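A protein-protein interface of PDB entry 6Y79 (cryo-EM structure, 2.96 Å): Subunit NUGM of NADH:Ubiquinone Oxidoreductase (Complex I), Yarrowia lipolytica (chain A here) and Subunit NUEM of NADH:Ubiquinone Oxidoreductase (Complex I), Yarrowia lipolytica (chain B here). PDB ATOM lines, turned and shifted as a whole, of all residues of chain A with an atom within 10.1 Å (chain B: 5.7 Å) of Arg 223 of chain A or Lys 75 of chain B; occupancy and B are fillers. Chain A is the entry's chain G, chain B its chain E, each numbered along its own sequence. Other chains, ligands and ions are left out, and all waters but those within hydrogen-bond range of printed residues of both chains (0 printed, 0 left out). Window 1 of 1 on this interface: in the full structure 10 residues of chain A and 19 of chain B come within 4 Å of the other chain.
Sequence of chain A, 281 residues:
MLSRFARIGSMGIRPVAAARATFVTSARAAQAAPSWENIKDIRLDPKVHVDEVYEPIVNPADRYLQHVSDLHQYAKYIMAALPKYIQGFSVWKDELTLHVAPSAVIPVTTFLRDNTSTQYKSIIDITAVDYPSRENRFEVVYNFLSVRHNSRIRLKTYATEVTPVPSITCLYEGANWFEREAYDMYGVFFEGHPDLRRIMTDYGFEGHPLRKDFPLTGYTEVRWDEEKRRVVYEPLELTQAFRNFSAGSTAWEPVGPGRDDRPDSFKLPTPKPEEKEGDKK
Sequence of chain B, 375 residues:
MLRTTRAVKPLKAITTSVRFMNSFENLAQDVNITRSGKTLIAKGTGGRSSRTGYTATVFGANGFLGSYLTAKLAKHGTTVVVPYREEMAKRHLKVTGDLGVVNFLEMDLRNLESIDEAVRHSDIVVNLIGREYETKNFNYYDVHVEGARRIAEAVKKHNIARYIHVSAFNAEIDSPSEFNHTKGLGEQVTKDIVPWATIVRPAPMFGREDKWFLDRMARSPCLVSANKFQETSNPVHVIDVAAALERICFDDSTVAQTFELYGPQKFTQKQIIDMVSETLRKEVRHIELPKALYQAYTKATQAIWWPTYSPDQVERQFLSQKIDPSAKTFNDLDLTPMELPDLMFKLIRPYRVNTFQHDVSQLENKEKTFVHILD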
ATOM      1  N   THR A 220     -22.338 -18.738  -3.815  1.00  0.00           N
ATOM      2  CA  THR A 220     -21.021 -18.266  -4.204  1.00  0.00           C
ATOM      3  C   THR A 220     -19.955 -19.305  -3.887  1.00  0.00           C
ATOM      4  O   THR A 220     -20.183 -20.277  -3.168  1.00  0.00           O
ATOM      5  CB  THR A 220     -20.664 -16.954  -3.494  1.00  0.00           C
ATOM      6  OG1 THR A 220     -20.547 -17.186  -2.088  1.00  0.00           O
ATOM      7  CG2 THR A 220     -21.716 -15.894  -3.737  1.00  0.00           C
ATOM      8  N   GLU A 221     -18.773 -19.061  -4.442  1.00  0.00           N
ATOM      9  CA  GLU A 221     -17.581 -19.858  -4.208  1.00  0.00           C
ATOM     10  C   GLU A 221     -16.380 -18.926  -4.204  1.00  0.00           C
ATOM     11  O   GLU A 221     -16.480 -17.753  -4.552  1.00  0.00           O
ATOM     12  CB  GLU A 221     -17.422 -20.953  -5.263  1.00  0.00           C
ATOM     13  CG  GLU A 221     -17.253 -20.421  -6.661  1.00  0.00           C
ATOM     14  CD  GLU A 221     -17.131 -21.518  -7.684  1.00  0.00           C
ATOM     15  OE1 GLU A 221     -17.217 -22.698  -7.291  1.00  0.00           O
ATOM     16  OE2 GLU A 221     -16.944 -21.204  -8.882  1.00  0.00           O
ATOM     17  N   VAL A 222     -15.230 -19.463  -3.812  1.00  0.00           N
ATOM     18  CA  VAL A 222     -14.021 -18.687  -3.553  1.00  0.00           C
ATOM     19  C   VAL A 222     -12.894 -19.250  -4.404  1.00  0.00           C
ATOM     20  O   VAL A 222     -12.743 -20.471  -4.502  1.00  0.00           O
ATOM     21  CB  VAL A 222     -13.646 -18.740  -2.058  1.00  0.00           C
ATOM     22  CG1 VAL A 222     -12.343 -18.035  -1.773  1.00  0.00           C
ATOM     23  CG2 VAL A 222     -14.733 -18.138  -1.229  1.00  0.00           C
ATOM     24  N   ARG A 223     -12.111 -18.371  -5.032  1.00  0.00           N
ATOM     25  CA  ARG A 223     -10.835 -18.820  -5.578  1.00  0.00           C
ATOM     26  C   ARG A 223      -9.813 -17.707  -5.427  1.00  0.00           C
ATOM     27  O   ARG A 223     -10.144 -16.597  -5.031  1.00  0.00           O
ATOM     28  CB  ARG A 223     -10.957 -19.262  -7.036  1.00  0.00           C
ATOM     29  CG  ARG A 223     -11.267 -18.166  -8.001  1.00  0.00           C
ATOM     30  CD  ARG A 223     -11.228 -18.697  -9.409  1.00  0.00           C
ATOM     31  NE  ARG A 223     -11.632 -17.680 -10.367  1.00  0.00           N
ATOM     32  CZ  ARG A 223     -10.795 -16.846 -10.966  1.00  0.00           C
ATOM     33  NH1 ARG A 223     -11.264 -15.948 -11.814  1.00  0.00           N
ATOM     34  NH2 ARG A 223      -9.498 -16.904 -10.714  1.00  0.00           N
ATOM     35  N   TRP A 224      -8.554 -18.022  -5.713  1.00  0.00           N
ATOM     36  CA  TRP A 224      -7.501 -17.011  -5.758  1.00  0.00           C
ATOM     37  C   TRP A 224      -7.420 -16.483  -7.177  1.00  0.00           C
ATOM     38  O   TRP A 224      -7.085 -17.226  -8.105  1.00  0.00           O
ATOM     39  CB  TRP A 224      -6.152 -17.572  -5.324  1.00  0.00           C
ATOM     40  CG  TRP A 224      -5.021 -16.587  -5.325  1.00  0.00           C
ATOM     41  CD1 TRP A 224      -4.058 -16.440  -6.276  1.00  0.00           C
ATOM     42  CD2 TRP A 224      -4.722 -15.636  -4.307  1.00  0.00           C
ATOM     43  NE1 TRP A 224      -3.185 -15.444  -5.917  1.00  0.00           N
ATOM     44  CE2 TRP A 224      -3.574 -14.935  -4.709  1.00  0.00           C
ATOM     45  CE3 TRP A 224      -5.317 -15.307  -3.094  1.00  0.00           C
ATOM     46  CZ2 TRP A 224      -3.015 -13.926  -3.940  1.00  0.00           C
ATOM     47  CZ3 TRP A 224      -4.777 -14.304  -2.346  1.00  0.00           C
ATOM     48  CH2 TRP A 224      -3.629 -13.629  -2.759  1.00  0.00           C
ATOM     49  N   ASP A 225      -7.756 -15.213  -7.352  1.00  0.00           N
ATOM     50  CA  ASP A 225      -7.479 -14.539  -8.607  1.00  0.00           C
ATOM     51  C   ASP A 225      -6.013 -14.132  -8.628  1.00  0.00           C
ATOM     52  O   ASP A 225      -5.518 -13.535  -7.669  1.00  0.00           O
ATOM     53  CB  ASP A 225      -8.382 -13.322  -8.734  1.00  0.00           C
ATOM     54  CG  ASP A 225      -8.264 -12.647 -10.067  1.00  0.00           C
ATOM     55  OD1 ASP A 225      -8.872 -13.122 -11.046  1.00  0.00           O
ATOM     56  OD2 ASP A 225      -7.550 -11.636 -10.132  1.00  0.00           O
ATOM     57  N   GLU A 226      -5.299 -14.488  -9.698  1.00  0.00           N
ATOM     58  CA  GLU A 226      -3.895 -14.094  -9.753  1.00  0.00           C
ATOM     59  C   GLU A 226      -3.758 -12.650 -10.217  1.00  0.00           C
ATOM     60  O   GLU A 226      -2.831 -11.943  -9.798  1.00  0.00           O
ATOM     61  CB  GLU A 226      -3.087 -15.031 -10.659  1.00  0.00           C
ATOM     62  CG  GLU A 226      -1.573 -14.797 -10.523  1.00  0.00           C
ATOM     63  CD  GLU A 226      -0.706 -15.676 -11.394  1.00  0.00           C
ATOM     64  OE1 GLU A 226      -1.230 -16.549 -12.091  1.00  0.00           O
ATOM     65  OE2 GLU A 226       0.525 -15.461 -11.424  1.00  0.00           O
ATOM     66  N   GLU A 227      -4.698 -12.187 -11.045  1.00  0.00           N
ATOM     67  CA  GLU A 227      -4.668 -10.817 -11.548  1.00  0.00           C
ATOM     68  C   GLU A 227      -4.827  -9.803 -10.415  1.00  0.00           C
ATOM     69  O   GLU A 227      -3.996  -8.904 -10.255  1.00  0.00           O
ATOM     70  CB  GLU A 227      -5.749 -10.637 -12.618  1.00  0.00           C
ATOM     71  CG  GLU A 227      -6.194  -9.209 -12.839  1.00  0.00           C
ATOM     72  CD  GLU A 227      -7.349  -9.104 -13.807  1.00  0.00           C
ATOM     73  OE1 GLU A 227      -7.985 -10.139 -14.087  1.00  0.00           O
ATOM     74  OE2 GLU A 227      -7.619  -7.986 -14.293  1.00  0.00           O
ATOM     75  N   LYS A 228      -5.856  -9.960  -9.582  1.00  0.00           N
ATOM     76  CA  LYS A 228      -6.057  -9.014  -8.491  1.00  0.00           C
ATOM     77  C   LYS A 228      -5.224  -9.316  -7.255  1.00  0.00           C
ATOM     78  O   LYS A 228      -5.198  -8.475  -6.348  1.00  0.00           O
ATOM     79  CB  LYS A 228      -7.525  -8.961  -8.084  1.00  0.00           C
ATOM     80  CG  LYS A 228      -8.449  -8.647  -9.218  1.00  0.00           C
ATOM     81  CD  LYS A 228      -9.873  -8.634  -8.756  1.00  0.00           C
ATOM     82  CE  LYS A 228     -10.796  -8.872  -9.924  1.00  0.00           C
ATOM     83  NZ  LYS A 228     -12.213  -8.791  -9.500  1.00  0.00           N
ATOM     84  N   ARG A 229      -4.566 -10.481  -7.204  1.00  0.00           N
ATOM     85  CA  ARG A 229      -3.755 -10.934  -6.064  1.00  0.00           C
ATOM     86  C   ARG A 229      -4.562 -10.957  -4.765  1.00  0.00           C
ATOM     87  O   ARG A 229      -4.078 -10.566  -3.701  1.00  0.00           O
ATOM     88  CB  ARG A 229      -2.480 -10.098  -5.906  1.00  0.00           C
ATOM     89  CG  ARG A 229      -1.549 -10.146  -7.110  1.00  0.00           C
ATOM     90  CD  ARG A 229      -0.785 -11.455  -7.170  1.00  0.00           C
ATOM     91  NE  ARG A 229       0.108 -11.518  -8.322  1.00  0.00           N
ATOM     92  CZ  ARG A 229       1.387 -11.160  -8.293  1.00  0.00           C
ATOM     93  NH1 ARG A 229       1.926 -10.713  -7.168  1.00  0.00           N
ATOM     94  NH2 ARG A 229       2.130 -11.251  -9.387  1.00  0.00           N
ATOM     95  N   ARG A 230      -5.809 -11.411  -4.860  1.00  0.00           N
ATOM     96  CA  ARG A 230      -6.655 -11.644  -3.700  1.00  0.00           C
ATOM     97  C   ARG A 230      -7.577 -12.809  -4.023  1.00  0.00           C
ATOM     98  O   ARG A 230      -7.619 -13.291  -5.159  1.00  0.00           O
ATOM     99  CB  ARG A 230      -7.453 -10.396  -3.319  1.00  0.00           C
ATOM    100  CG  ARG A 230      -8.461  -9.960  -4.359  1.00  0.00           C
ATOM    101  CD  ARG A 230      -9.230  -8.753  -3.869  1.00  0.00           C
ATOM    102  NE  ARG A 230     -10.118  -8.215  -4.893  1.00  0.00           N
ATOM    103  CZ  ARG A 230     -11.390  -8.568  -5.030  1.00  0.00           C
ATOM    104  NH1 ARG A 230     -12.127  -8.032  -5.988  1.00  0.00           N
ATOM    105  NH2 ARG A 230     -11.923  -9.460  -4.209  1.00  0.00           N
ATOM    106  N   VAL A 231      -8.312 -13.282  -3.016  1.00  0.00           N
ATOM    107  CA  VAL A 231      -9.377 -14.232  -3.309  1.00  0.00           C
ATOM    108  C   VAL A 231     -10.591 -13.456  -3.803  1.00  0.00           C
ATOM    109  O   VAL A 231     -10.887 -12.346  -3.345  1.00  0.00           O
ATOM    110  CB  VAL A 231      -9.703 -15.148  -2.102  1.00  0.00           C
ATOM    111  CG1 VAL A 231      -8.463 -15.797  -1.548  1.00  0.00           C
ATOM    112  CG2 VAL A 231     -10.446 -14.462  -1.000  1.00  0.00           C
ATOM    113  N   VAL A 232     -11.241 -14.000  -4.813  1.00  0.00           N
ATOM    114  CA  VAL A 232     -12.462 -13.438  -5.351  1.00  0.00           C
ATOM    115  C   VAL A 232     -13.596 -14.397  -5.049  1.00  0.00           C
ATOM    116  O   VAL A 232     -13.405 -15.613  -4.906  1.00  0.00           O
ATOM    117  CB  VAL A 232     -12.379 -13.163  -6.865  1.00  0.00           C
ATOM    118  CG1 VAL A 232     -11.454 -12.001  -7.131  1.00  0.00           C
ATOM    119  CG2 VAL A 232     -11.932 -14.399  -7.607  1.00  0.00           C
ATOM    120  N   TYR A 233     -14.785 -13.822  -4.935  1.00  0.00           N
ATOM    121  CA  TYR A 233     -16.005 -14.548  -4.635  1.00  0.00           C
ATOM    122  C   TYR A 233     -16.850 -14.503  -5.895  1.00  0.00           C
ATOM    123  O   TYR A 233     -17.190 -13.422  -6.376  1.00  0.00           O
ATOM    124  CB  TYR A 233     -16.755 -13.935  -3.448  1.00  0.00           C
ATOM    125  CG  TYR A 233     -16.093 -14.042  -2.078  1.00  0.00           C
ATOM    126  CD1 TYR A 233     -14.828 -14.581  -1.909  1.00  0.00           C
ATOM    127  CD2 TYR A 233     -16.760 -13.626  -0.949  1.00  0.00           C
ATOM    128  CE1 TYR A 233     -14.241 -14.666  -0.666  1.00  0.00           C
ATOM    129  CE2 TYR A 233     -16.183 -13.715   0.303  1.00  0.00           C
ATOM    130  CZ  TYR A 233     -14.927 -14.242   0.433  1.00  0.00           C
ATOM    131  OH  TYR A 233     -14.335 -14.351   1.666  1.00  0.00           O
ATOM    132  N   GLU A 234     -17.169 -15.666  -6.431  1.00  0.00           N
ATOM    133  CA  GLU A 234     -17.800 -15.812  -7.729  1.00  0.00           C
ATOM    134  C   GLU A 234     -19.115 -16.551  -7.572  1.00  0.00           C
ATOM    135  O   GLU A 234     -19.350 -17.183  -6.540  1.00  0.00           O
ATOM    136  CB  GLU A 234     -16.872 -16.577  -8.679  1.00  0.00           C
ATOM    137  CG  GLU A 234     -15.776 -15.718  -9.234  1.00  0.00           C
ATOM    138  CD  GLU A 234     -14.919 -16.457 -10.221  1.00  0.00           C
ATOM    139  OE1 GLU A 234     -13.688 -16.425 -10.057  1.00  0.00           O
ATOM    140  OE2 GLU A 234     -15.471 -17.067 -11.158  1.00  0.00           O
ATOM    141  N   PRO A 235     -20.011 -16.463  -8.554  1.00  0.00           N
ATOM    142  CA  PRO A 235     -21.172 -17.353  -8.552  1.00  0.00           C
ATOM    143  C   PRO A 235     -20.748 -18.801  -8.711  1.00  0.00           C
ATOM    144  O   PRO A 235     -19.729 -19.126  -9.319  1.00  0.00           O
ATOM    145  CB  PRO A 235     -22.002 -16.877  -9.747  1.00  0.00           C
ATOM    146  CG  PRO A 235     -21.104 -16.027 -10.529  1.00  0.00           C
ATOM    147  CD  PRO A 235     -20.169 -15.404  -9.559  1.00  0.00           C
ATOM    148  N   LEU A 236     -21.559 -19.674  -8.135  1.00  0.00           N
ATOM    149  CA  LEU A 236     -21.129 -21.029  -7.850  1.00  0.00           C
ATOM    150  C   LEU A 236     -21.198 -21.913  -9.082  1.00  0.00           C
ATOM    151  O   LEU A 236     -22.088 -21.775  -9.923  1.00  0.00           O
ATOM    152  CB  LEU A 236     -21.991 -21.609  -6.745  1.00  0.00           C
ATOM    153  CG  LEU A 236     -21.792 -23.032  -6.253  1.00  0.00           C
ATOM    154  CD1 LEU A 236     -20.412 -23.242  -5.693  1.00  0.00           C
ATOM    155  CD2 LEU A 236     -22.807 -23.212  -5.202  1.00  0.00           C
ATOM    156  N   GLU A 237     -20.240 -22.829  -9.171  1.00  0.00           N
ATOM    157  CA  GLU A 237     -20.173 -23.780 -10.263  1.00  0.00           C
ATOM    158  C   GLU A 237     -19.400 -24.991  -9.775  1.00  0.00           C
ATOM    159  O   GLU A 237     -18.353 -24.836  -9.141  1.00  0.00           O
ATOM    160  CB  GLU A 237     -19.498 -23.142 -11.459  1.00  0.00           C
ATOM    161  CG  GLU A 237     -19.723 -23.857 -12.721  1.00  0.00           C
ATOM    162  CD  GLU A 237     -18.934 -23.249 -13.819  1.00  0.00           C
ATOM    163  OE1 GLU A 237     -18.264 -22.225 -13.585  1.00  0.00           O
ATOM    164  OE2 GLU A 237     -18.968 -23.810 -14.915  1.00  0.00           O
ATOM    165  N   GLY B  47     -16.502 -19.286 -16.134  1.00  0.00           N
ATOM    166  CA  GLY B  47     -15.902 -19.486 -14.839  1.00  0.00           C
ATOM    167  C   GLY B  47     -14.999 -20.699 -14.770  1.00  0.00           C
ATOM    168  O   GLY B  47     -14.569 -21.260 -15.780  1.00  0.00           O
ATOM    169  N   ARG B  48     -14.728 -21.115 -13.531  1.00  0.00           N
ATOM    170  CA  ARG B  48     -13.629 -22.037 -13.259  1.00  0.00           C
ATOM    171  C   ARG B  48     -13.950 -23.446 -13.726  1.00  0.00           C
ATOM    172  O   ARG B  48     -13.139 -24.083 -14.405  1.00  0.00           O
ATOM    173  CB  ARG B  48     -13.314 -22.032 -11.766  1.00  0.00           C
ATOM    174  CG  ARG B  48     -12.216 -22.980 -11.356  1.00  0.00           C
ATOM    175  CD  ARG B  48     -11.850 -22.773  -9.906  1.00  0.00           C
ATOM    176  NE  ARG B  48     -10.703 -23.580  -9.512  1.00  0.00           N
ATOM    177  CZ  ARG B  48      -9.453 -23.141  -9.507  1.00  0.00           C
ATOM    178  NH1 ARG B  48      -8.469 -23.943  -9.136  1.00  0.00           N
ATOM    179  NH2 ARG B  48      -9.190 -21.896  -9.868  1.00  0.00           N
ATOM    180  N   THR B  70      -1.625 -16.524 -18.881  1.00  0.00           N
ATOM    181  CA  THR B  70      -2.337 -17.768 -18.622  1.00  0.00           C
ATOM    182  C   THR B  70      -3.169 -17.726 -17.347  1.00  0.00           C
ATOM    183  O   THR B  70      -3.927 -18.666 -17.101  1.00  0.00           O
ATOM    184  CB  THR B  70      -1.393 -18.958 -18.557  1.00  0.00           C
ATOM    185  OG1 THR B  70      -2.176 -20.149 -18.448  1.00  0.00           O
ATOM    186  CG2 THR B  70      -0.531 -18.866 -17.342  1.00  0.00           C
ATOM    187  N   ALA B  71      -3.053 -16.682 -16.525  1.00  0.00           N
ATOM    188  CA  ALA B  71      -4.075 -16.449 -15.516  1.00  0.00           C
ATOM    189  C   ALA B  71      -5.377 -16.035 -16.180  1.00  0.00           C
ATOM    190  O   ALA B  71      -6.459 -16.488 -15.791  1.00  0.00           O
ATOM    191  CB  ALA B  71      -3.610 -15.386 -14.522  1.00  0.00           C
ATOM    192  N   LYS B  72      -5.287 -15.168 -17.192  1.00  0.00           N
ATOM    193  CA  LYS B  72      -6.477 -14.775 -17.934  1.00  0.00           C
ATOM    194  C   LYS B  72      -6.953 -15.869 -18.879  1.00  0.00           C
ATOM    195  O   LYS B  72      -8.121 -15.874 -19.276  1.00  0.00           O
ATOM    196  CB  LYS B  72      -6.201 -13.507 -18.721  1.00  0.00           C
ATOM    197  CG  LYS B  72      -5.918 -12.286 -17.902  1.00  0.00           C
ATOM    198  CD  LYS B  72      -5.668 -11.153 -18.851  1.00  0.00           C
ATOM    199  CE  LYS B  72      -5.554  -9.863 -18.109  1.00  0.00           C
ATOM    200  NZ  LYS B  72      -6.770  -9.587 -17.318  1.00  0.00           N
ATOM    201  N   LEU B  73      -6.062 -16.779 -19.265  1.00  0.00           N
ATOM    202  CA  LEU B  73      -6.405 -17.823 -20.223  1.00  0.00           C
ATOM    203  C   LEU B  73      -7.087 -19.001 -19.540  1.00  0.00           C
ATOM    204  O   LEU B  73      -8.117 -19.487 -20.016  1.00  0.00           O
ATOM    205  CB  LEU B  73      -5.141 -18.274 -20.948  1.00  0.00           C
ATOM    206  CG  LEU B  73      -5.171 -18.980 -22.295  1.00  0.00           C
ATOM    207  CD1 LEU B  73      -6.005 -18.207 -23.293  1.00  0.00           C
ATOM    208  CD2 LEU B  73      -3.734 -19.072 -22.776  1.00  0.00           C
ATOM    209  N   ALA B  74      -6.541 -19.458 -18.414  1.00  0.00           N
ATOM    210  CA  ALA B  74      -7.111 -20.562 -17.653  1.00  0.00           C
ATOM    211  C   ALA B  74      -8.260 -20.137 -16.755  1.00  0.00           C
ATOM    212  O   ALA B  74      -8.794 -20.973 -16.024  1.00  0.00           O
ATOM    213  CB  ALA B  74      -6.027 -21.225 -16.804  1.00  0.00           C
ATOM    214  N   LYS B  75      -8.636 -18.860 -16.783  1.00  0.00           N
ATOM    215  CA  LYS B  75      -9.743 -18.370 -15.970  1.00  0.00           C
ATOM    216  C   LYS B  75     -11.075 -18.911 -16.466  1.00  0.00           C
ATOM    217  O   LYS B  75     -11.973 -19.195 -15.667  1.00  0.00           O
ATOM    218  CB  LYS B  75      -9.732 -16.844 -15.995  1.00  0.00           C
ATOM    219  CG  LYS B  75     -10.769 -16.133 -15.167  1.00  0.00           C
ATOM    220  CD  LYS B  75     -10.453 -14.652 -15.207  1.00  0.00           C
ATOM    221  CE  LYS B  75     -11.443 -13.809 -14.441  1.00  0.00           C
ATOM    222  NZ  LYS B  75     -11.044 -12.372 -14.504  1.00  0.00           N
ATOM    223  N   HIS B  76     -11.211 -19.076 -17.778  1.00  0.00           N
ATOM    224  CA  HIS B  76     -12.456 -19.512 -18.388  1.00  0.00           C
ATOM    225  C   HIS B  76     -12.459 -20.971 -18.782  1.00  0.00           C
ATOM    226  O   HIS B  76     -13.485 -21.464 -19.250  1.00  0.00           O
ATOM    227  CB  HIS B  76     -12.761 -18.654 -19.607  1.00  0.00           C
ATOM    228  CG  HIS B  76     -13.084 -17.252 -19.246  1.00  0.00           C
ATOM    229  ND1 HIS B  76     -14.226 -16.925 -18.554  1.00  0.00           N
ATOM    230  CD2 HIS B  76     -12.404 -16.098 -19.427  1.00  0.00           C
ATOM    231  CE1 HIS B  76     -14.247 -15.625 -18.336  1.00  0.00           C
ATOM    232  NE2 HIS B  76     -13.155 -15.099 -18.860  1.00  0.00           N
ATOM    233  N   GLY B  77     -11.350 -21.669 -18.608  1.00  0.00           N
ATOM    234  CA  GLY B  77     -11.295 -23.073 -18.911  1.00  0.00           C
ATOM    235  C   GLY B  77     -10.618 -23.431 -20.205  1.00  0.00           C
ATOM    236  O   GLY B  77     -10.845 -24.532 -20.711  1.00  0.00           O
ATOM    237  N   THR B  78      -9.819 -22.537 -20.767  1.00  0.00           N
ATOM    238  CA  THR B  78      -8.964 -22.905 -21.881  1.00  0.00           C
ATOM    239  C   THR B  78      -7.861 -23.816 -21.367  1.00  0.00           C
ATOM    240  O   THR B  78      -7.192 -23.488 -20.388  1.00  0.00           O
ATOM    241  CB  THR B  78      -8.378 -21.652 -22.521  1.00  0.00           C
ATOM    242  OG1 THR B  78      -9.444 -20.819 -22.991  1.00  0.00           O
ATOM    243  CG2 THR B  78      -7.464 -22.009 -23.678  1.00  0.00           C
ATOM    244  N   THR B  96      -4.205 -21.183 -10.861  1.00  0.00           N
ATOM    245  CA  THR B  96      -4.968 -20.335 -11.767  1.00  0.00           C
ATOM    246  C   THR B  96      -6.078 -21.052 -12.512  1.00  0.00           C
ATOM    247  O   THR B  96      -7.046 -20.403 -12.920  1.00  0.00           O
ATOM    248  CB  THR B  96      -4.045 -19.716 -12.815  1.00  0.00           C
ATOM    249  OG1 THR B  96      -3.803 -20.674 -13.851  1.00  0.00           O
ATOM    250  CG2 THR B  96      -2.746 -19.332 -12.190  1.00  0.00           C
ATOM    251  N   GLY B  97      -5.964 -22.361 -12.725  1.00  0.00           N
ATOM    252  CA  GLY B  97      -6.901 -23.084 -13.549  1.00  0.00           C
ATOM    253  C   GLY B  97      -7.621 -24.164 -12.763  1.00  0.00           C
ATOM    254  O   GLY B  97      -7.257 -24.503 -11.634  1.00  0.00           O
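The side-chain amino group of Lys 72 of chain B lies within salt-bridge range of the side-chain carboxylate of Glu 227 of chain A (3.5 Å). OE1 of Glu 227 of chain A lies within salt-bridge range of NZ of Lys 75 of chain B (3.8 Å).
The backbone carbonyl oxygen (O) of Arg 223 of chain A lies within hydrogen-bond range of the backbone NH (N) of Val 232 of chain A, at 2.8 Å. The guanidinium group (NH1) of Arg 223 of chain A is in salt-bridge range of the side-chain carboxylate (OD1) of Asp 225 of chain A (3.8 Å). The backbone carbonyl oxygen (O) of Glu 226 of chain A sits at hydrogen-bond distance from the guanidinium group (NE) of Arg 229 of chain A (3.3 Å). The guanidinium group (NH1) of Arg 48 of chain B is in hydrogen-bond range of the backbone carbonyl oxygen (O) of Gly 97 of chain B (2.8 Å). The guanidinium group (NE) of Arg 223 of chain A lies within salt-bridge range of the side-chain carboxylate (OE1) of Glu 234 of chain A (2.4 Å). The side-chain carboxylate (OD2) of Asp 225 of chain A lies within hydrogen-bond range of the backbone NH (N) of Glu 227 of chain A (3.0 Å).
Among the printed residues, merely in contact across the chains: Arg 223 of chain A with Arg 48 of chain B (3.8 Å), Arg 223 of chain A with Lys 75 of chain B (3.4 Å), Glu 226 of chain A with Ala 71 of chain B (3.6 Å), Glu 226 of chain A with Thr 96 of chain B (3.2 Å), Glu 237 of chain A with Gly 47 of chain B (3.8 Å) and Glu 237 of chain A with Arg 48 of chain B (3.7 Å).
Arg 223 of chain A touches two residues of chain B. Lys 75 of chain B touches two residues of chain A. Of chain A, only Arg 223 (3.8 Å) and Glu 237 (3.7 Å) come within 4 Å of Arg 48 of chain B. No residue of chain A comes within 4 Å of Ala 74 of chain B. No residue of chain A comes within 4 Å of His 76 of chain B. Of the printed residues of chain A, Ala 71 of chain B touches Glu 226. Printed residues of chain B within 4 Å of Glu 237 of chain A: Gly 47 and Arg 48. Printed residues of chain A within 4 Å of Thr 96 of chain B: Glu 226. The nearest residue of chain A that does not touch Lys 75 of chain B is Asp 225 of chain A (4.2 Å).
Of the 13 printed residues of chain B, 6 touch a printed residue of chain A. Printed residues of chain B that touch a printed residue of chain A: Gly 47, Arg 48, Ala 71, Lys 72, Lys 75 and Thr 96. Hydrophobic or aromatic side chains of chain B within 4 Å of the printed part of chain A: Ala 71. Among the printed residues, Asp or Glu carboxylates within 4 Å of a Lys or Arg side-chain nitrogen of the other chain: Glu 227 of chain A with Lys 72 of chain B and Glu 227 of chain A with Lys 75 of chain B.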
